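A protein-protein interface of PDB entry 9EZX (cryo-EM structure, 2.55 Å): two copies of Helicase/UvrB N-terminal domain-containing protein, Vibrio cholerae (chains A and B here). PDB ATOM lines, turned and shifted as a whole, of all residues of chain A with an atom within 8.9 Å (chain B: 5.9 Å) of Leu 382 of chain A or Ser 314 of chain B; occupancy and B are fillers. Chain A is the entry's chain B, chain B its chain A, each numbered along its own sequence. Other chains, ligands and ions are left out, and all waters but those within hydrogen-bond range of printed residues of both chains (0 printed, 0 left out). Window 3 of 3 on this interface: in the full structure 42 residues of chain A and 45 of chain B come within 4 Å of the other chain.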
ATOM      1  N   PHE A 343       3.444  22.298  30.882  1.00  0.00           N
ATOM      2  CA  PHE A 343       3.192  21.950  29.493  1.00  0.00           C
ATOM      3  C   PHE A 343       4.217  20.935  29.012  1.00  0.00           C
ATOM      4  O   PHE A 343       5.370  20.945  29.450  1.00  0.00           O
ATOM      5  CB  PHE A 343       3.254  23.189  28.600  1.00  0.00           C
ATOM      6  CG  PHE A 343       2.430  24.338  29.092  1.00  0.00           C
ATOM      7  CD1 PHE A 343       1.250  24.124  29.775  1.00  0.00           C
ATOM      8  CD2 PHE A 343       2.837  25.638  28.863  1.00  0.00           C
ATOM      9  CE1 PHE A 343       0.494  25.183  30.223  1.00  0.00           C
ATOM     10  CE2 PHE A 343       2.085  26.697  29.308  1.00  0.00           C
ATOM     11  CZ  PHE A 343       0.914  26.470  29.989  1.00  0.00           C
ATOM     12  N   SER A 379       6.948  29.176  25.432  1.00  0.00           N
ATOM     13  CA  SER A 379       5.747  28.607  26.027  1.00  0.00           C
ATOM     14  C   SER A 379       4.535  29.303  25.428  1.00  0.00           C
ATOM     15  O   SER A 379       4.395  30.524  25.548  1.00  0.00           O
ATOM     16  CB  SER A 379       5.758  28.768  27.546  1.00  0.00           C
ATOM     17  OG  SER A 379       6.911  28.179  28.114  1.00  0.00           O
ATOM     18  N   ASP A 380       3.666  28.530  24.787  1.00  0.00           N
ATOM     19  CA  ASP A 380       2.442  29.061  24.191  1.00  0.00           C
ATOM     20  C   ASP A 380       1.300  28.790  25.160  1.00  0.00           C
ATOM     21  O   ASP A 380       0.708  27.710  25.156  1.00  0.00           O
ATOM     22  CB  ASP A 380       2.188  28.428  22.829  1.00  0.00           C
ATOM     23  CG  ASP A 380       1.073  29.112  22.068  1.00  0.00           C
ATOM     24  OD1 ASP A 380       0.256  29.809  22.704  1.00  0.00           O
ATOM     25  OD2 ASP A 380       1.011  28.954  20.831  1.00  0.00           O
ATOM     26  N   PHE A 381       0.988  29.778  26.000  1.00  0.00           N
ATOM     27  CA  PHE A 381      -0.069  29.600  26.984  1.00  0.00           C
ATOM     28  C   PHE A 381      -1.430  29.397  26.337  1.00  0.00           C
ATOM     29  O   PHE A 381      -2.330  28.847  26.979  1.00  0.00           O
ATOM     30  CB  PHE A 381      -0.112  30.798  27.927  1.00  0.00           C
ATOM     31  CG  PHE A 381       1.054  30.863  28.865  1.00  0.00           C
ATOM     32  CD1 PHE A 381       1.017  30.208  30.080  1.00  0.00           C
ATOM     33  CD2 PHE A 381       2.190  31.574  28.527  1.00  0.00           C
ATOM     34  CE1 PHE A 381       2.089  30.262  30.943  1.00  0.00           C
ATOM     35  CE2 PHE A 381       3.265  31.632  29.387  1.00  0.00           C
ATOM     36  CZ  PHE A 381       3.213  30.976  30.596  1.00  0.00           C
ATOM     37  N   LEU A 382      -1.607  29.833  25.090  1.00  0.00           N
ATOM     38  CA  LEU A 382      -2.847  29.546  24.381  1.00  0.00           C
ATOM     39  C   LEU A 382      -2.933  28.070  24.015  1.00  0.00           C
ATOM     40  O   LEU A 382      -3.967  27.426  24.227  1.00  0.00           O
ATOM     41  CB  LEU A 382      -2.951  30.419  23.131  1.00  0.00           C
ATOM     42  CG  LEU A 382      -3.896  31.618  23.228  1.00  0.00           C
ATOM     43  CD1 LEU A 382      -5.339  31.156  23.364  1.00  0.00           C
ATOM     44  CD2 LEU A 382      -3.507  32.514  24.393  1.00  0.00           C
ATOM     45  N   ARG A 383      -1.852  27.514  23.466  1.00  0.00           N
ATOM     46  CA  ARG A 383      -1.817  26.098  23.128  1.00  0.00           C
ATOM     47  C   ARG A 383      -1.395  25.218  24.294  1.00  0.00           C
ATOM     48  O   ARG A 383      -1.485  23.992  24.181  1.00  0.00           O
ATOM     49  CB  ARG A 383      -0.871  25.854  21.952  1.00  0.00           C
ATOM     50  CG  ARG A 383      -1.585  25.679  20.627  1.00  0.00           C
ATOM     51  CD  ARG A 383      -0.621  25.336  19.509  1.00  0.00           C
ATOM     52  NE  ARG A 383       0.338  26.401  19.252  1.00  0.00           N
ATOM     53  CZ  ARG A 383       1.335  26.316  18.382  1.00  0.00           C
ATOM     54  NH1 ARG A 383       1.553  25.211  17.689  1.00  0.00           N
ATOM     55  NH2 ARG A 383       2.130  27.366  18.202  1.00  0.00           N
ATOM     56  N   ARG A 384      -0.942  25.800  25.401  1.00  0.00           N
ATOM     57  CA  ARG A 384      -0.495  25.025  26.555  1.00  0.00           C
ATOM     58  C   ARG A 384       0.596  24.036  26.158  1.00  0.00           C
ATOM     59  O   ARG A 384       0.589  22.875  26.571  1.00  0.00           O
ATOM     60  CB  ARG A 384      -1.666  24.297  27.212  1.00  0.00           C
ATOM     61  CG  ARG A 384      -2.753  25.211  27.723  1.00  0.00           C
ATOM     62  CD  ARG A 384      -3.911  24.415  28.278  1.00  0.00           C
ATOM     63  NE  ARG A 384      -4.913  25.272  28.897  1.00  0.00           N
ATOM     64  CZ  ARG A 384      -6.042  24.834  29.435  1.00  0.00           C
ATOM     65  NH1 ARG A 384      -6.348  23.547  29.450  1.00  0.00           N
ATOM     66  NH2 ARG A 384      -6.886  25.709  29.974  1.00  0.00           N
ATOM     67  N   LYS A 385       1.539  24.496  25.343  1.00  0.00           N
ATOM     68  CA  LYS A 385       2.658  23.684  24.893  1.00  0.00           C
ATOM     69  C   LYS A 385       3.943  24.491  24.953  1.00  0.00           C
ATOM     70  O   LYS A 385       3.930  25.712  24.771  1.00  0.00           O
ATOM     71  CB  LYS A 385       2.439  23.186  23.467  1.00  0.00           C
ATOM     72  CG  LYS A 385       1.836  21.804  23.386  1.00  0.00           C
ATOM     73  CD  LYS A 385       2.900  20.728  23.328  1.00  0.00           C
ATOM     74  CE  LYS A 385       2.349  19.452  22.731  1.00  0.00           C
ATOM     75  NZ  LYS A 385       2.982  18.249  23.315  1.00  0.00           N
ATOM     76  N   LEU A 387       7.199  24.982  22.883  1.00  0.00           N
ATOM     77  CA  LEU A 387       7.469  24.760  21.469  1.00  0.00           C
ATOM     78  C   LEU A 387       8.934  25.047  21.179  1.00  0.00           C
ATOM     79  O   LEU A 387       9.437  26.125  21.512  1.00  0.00           O
ATOM     80  CB  LEU A 387       6.566  25.639  20.607  1.00  0.00           C
ATOM     81  CG  LEU A 387       5.075  25.379  20.813  1.00  0.00           C
ATOM     82  CD1 LEU A 387       4.256  26.531  20.271  1.00  0.00           C
ATOM     83  CD2 LEU A 387       4.659  24.066  20.174  1.00  0.00           C
ATOM     84  N   ASP A 515       3.097  14.674  18.434  1.00  0.00           N
ATOM     85  CA  ASP A 515       2.975  16.057  18.967  1.00  0.00           C
ATOM     86  C   ASP A 515       3.751  16.246  20.278  1.00  0.00           C
ATOM     87  O   ASP A 515       3.733  17.375  20.746  1.00  0.00           O
ATOM     88  CB  ASP A 515       1.503  16.454  19.112  1.00  0.00           C
ATOM     89  CG  ASP A 515       0.763  15.798  20.263  1.00  0.00           C
ATOM     90  OD1 ASP A 515       1.027  14.611  20.537  1.00  0.00           O
ATOM     91  OD2 ASP A 515      -0.088  16.480  20.859  1.00  0.00           O
ATOM     92  N   LEU B 312      -3.042  19.089  29.236  1.00  0.00           N
ATOM     93  CA  LEU B 312      -3.025  18.781  27.817  1.00  0.00           C
ATOM     94  C   LEU B 312      -2.967  20.065  26.999  1.00  0.00           C
ATOM     95  O   LEU B 312      -3.284  21.155  27.484  1.00  0.00           O
ATOM     96  CB  LEU B 312      -4.264  17.983  27.416  1.00  0.00           C
ATOM     97  CG  LEU B 312      -4.331  16.523  27.850  1.00  0.00           C
ATOM     98  CD1 LEU B 312      -5.758  16.026  27.757  1.00  0.00           C
ATOM     99  CD2 LEU B 312      -3.419  15.672  26.997  1.00  0.00           C
ATOM    100  N   GLU B 313      -2.566  19.928  25.741  1.00  0.00           N
ATOM    101  CA  GLU B 313      -2.529  21.082  24.860  1.00  0.00           C
ATOM    102  C   GLU B 313      -3.912  21.337  24.265  1.00  0.00           C
ATOM    103  O   GLU B 313      -4.783  20.464  24.244  1.00  0.00           O
ATOM    104  CB  GLU B 313      -1.484  20.885  23.762  1.00  0.00           C
ATOM    105  CG  GLU B 313      -1.807  19.826  22.725  1.00  0.00           C
ATOM    106  CD  GLU B 313      -1.220  20.147  21.361  1.00  0.00           C
ATOM    107  OE1 GLU B 313      -0.872  21.320  21.116  1.00  0.00           O
ATOM    108  OE2 GLU B 313      -1.107  19.221  20.532  1.00  0.00           O
ATOM    109  N   SER B 314      -4.107  22.561  23.779  1.00  0.00           N
ATOM    110  CA  SER B 314      -5.405  23.014  23.302  1.00  0.00           C
ATOM    111  C   SER B 314      -5.600  22.779  21.810  1.00  0.00           C
ATOM    112  O   SER B 314      -6.336  23.534  21.165  1.00  0.00           O
ATOM    113  CB  SER B 314      -5.590  24.497  23.624  1.00  0.00           C
ATOM    114  OG  SER B 314      -5.524  24.725  25.020  1.00  0.00           O
ATOM    115  N   SER B 315      -4.961  21.759  21.249  1.00  0.00           N
ATOM    116  CA  SER B 315      -5.156  21.438  19.849  1.00  0.00           C
ATOM    117  C   SER B 315      -6.489  20.720  19.651  1.00  0.00           C
ATOM    118  O   SER B 315      -7.068  20.190  20.601  1.00  0.00           O
ATOM    119  CB  SER B 315      -4.012  20.568  19.341  1.00  0.00           C
ATOM    120  OG  SER B 315      -4.028  19.297  19.963  1.00  0.00           O
ATOM    121  N   PRO B 316      -7.035  20.622  18.411  1.00  0.00           N
ATOM    122  CA  PRO B 316      -8.272  19.859  18.163  1.00  0.00           C
ATOM    123  C   PRO B 316      -8.214  18.381  18.575  1.00  0.00           C
ATOM    124  O   PRO B 316      -9.270  17.804  18.742  1.00  0.00           O
ATOM    125  CB  PRO B 316      -8.454  19.917  16.640  1.00  0.00           C
ATOM    126  CG  PRO B 316      -7.741  21.178  16.236  1.00  0.00           C
ATOM    127  CD  PRO B 316      -6.551  21.244  17.167  1.00  0.00           C
ATOM    128  N   TYR B 318      -7.486  17.187  21.380  1.00  0.00           N
ATOM    129  CA  TYR B 318      -7.974  17.089  22.784  1.00  0.00           C
ATOM    130  C   TYR B 318      -9.253  17.893  22.980  1.00  0.00           C
ATOM    131  O   TYR B 318      -9.421  18.470  24.070  1.00  0.00           O
ATOM    132  CB  TYR B 318      -6.893  17.552  23.754  1.00  0.00           C
ATOM    133  CG  TYR B 318      -5.585  16.899  23.432  1.00  0.00           C
ATOM    134  CD1 TYR B 318      -5.331  15.605  23.842  1.00  0.00           C
ATOM    135  CD2 TYR B 318      -4.665  17.536  22.622  1.00  0.00           C
ATOM    136  CE1 TYR B 318      -4.151  14.974  23.510  1.00  0.00           C
ATOM    137  CE2 TYR B 318      -3.481  16.920  22.277  1.00  0.00           C
ATOM    138  CZ  TYR B 318      -3.231  15.644  22.730  1.00  0.00           C
ATOM    139  OH  TYR B 318      -2.072  15.050  22.393  1.00  0.00           O
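OE2 of Glu 313 of chain B sits at hydrogen-bond distance from OG of Ser 315 of chain B (3.0 Å).
The side-chain carboxylate (OD1) of Asp 380 of chain A is in hydrogen-bond range of the backbone NH (N) of Leu 382 of chain A, at 3.0 Å.
The side-chain carboxylate of Asp 380 of chain A is in salt-bridge range of the guanidinium group of Arg 383 of chain A (3.1 Å).
The backbone NH of Asp 380 of chain A is in hydrogen-bond range of the backbone carbonyl oxygen of Lys 385 of chain A (2.8 Å).
The side-chain amino group of Lys 385 of chain A lies within hydrogen-bond range of the backbone carbonyl oxygen of Asp 515 of chain A, 2.8 Å away.
Of the 10 printed residues of chain A, 5 touch a printed residue of chain B.
Hydrophobic or aromatic side chains of chain B within 4 Å of the printed part of chain A: Tyr 318.
Among the printed residues, 9 pairs touch across the chains.
Among the printed residues, merely in contact across the chains: Arg 383 of chain A with Glu 313 of chain B (3.1 Å), Arg 384 of chain A with Leu 312 of chain B (3.4 Å), Arg 384 of chain A with Glu 313 of chain B (3.98 Å), Arg 384 of chain A with Ser 314 of chain B (3.6 Å) and Lys 385 of chain A with Glu 313 of chain B (3.5 Å).
Phe 381 of chain A touches none of the printed residues of chain B.
Of chain B, only Ser 314 comes within 4 Å of Leu 382 of chain A.
Of the printed residues of chain B, Arg 383 of chain A touches Glu 313 and Ser 314.
Printed residues of chain B within 4 Å of Arg 384 of chain A: Leu 312 (3.4 Å), Glu 313 (3.98 Å) and Ser 314 (3.6 Å).
Of the printed residues of chain A, Leu 312 of chain B touches Arg 384 (3.4 Å).
Ser 314 of chain B touches just these residues of chain A: Leu 382, Arg 383 and Arg 384.
No residue of chain A comes within 4 Å of Ser 315 of chain B.
The nearest printed residue of chain B that does not touch Leu 382 of chain A is Glu 313 of chain B (6.1 Å).
No position is printed for both chains.
The side-chain hydroxyl (OG) of Ser 314 of chain B sits at hydrogen-bond distance from the backbone carbonyl oxygen (O) of Leu 382 of chain A (3.2 Å).
N of Ser 314 of chain B sits at hydrogen-bond distance from O of Arg 383 of chain A, 3.0 Å away.
The side-chain hydroxyl of Tyr 318 of chain B is in hydrogen-bond range of the side-chain carboxylate of Asp 515 of chain A, at 2.9 Å.
OE2 of Glu 313 of chain B sits close to OD2 of Asp 515 of chain A (2.9 Å).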
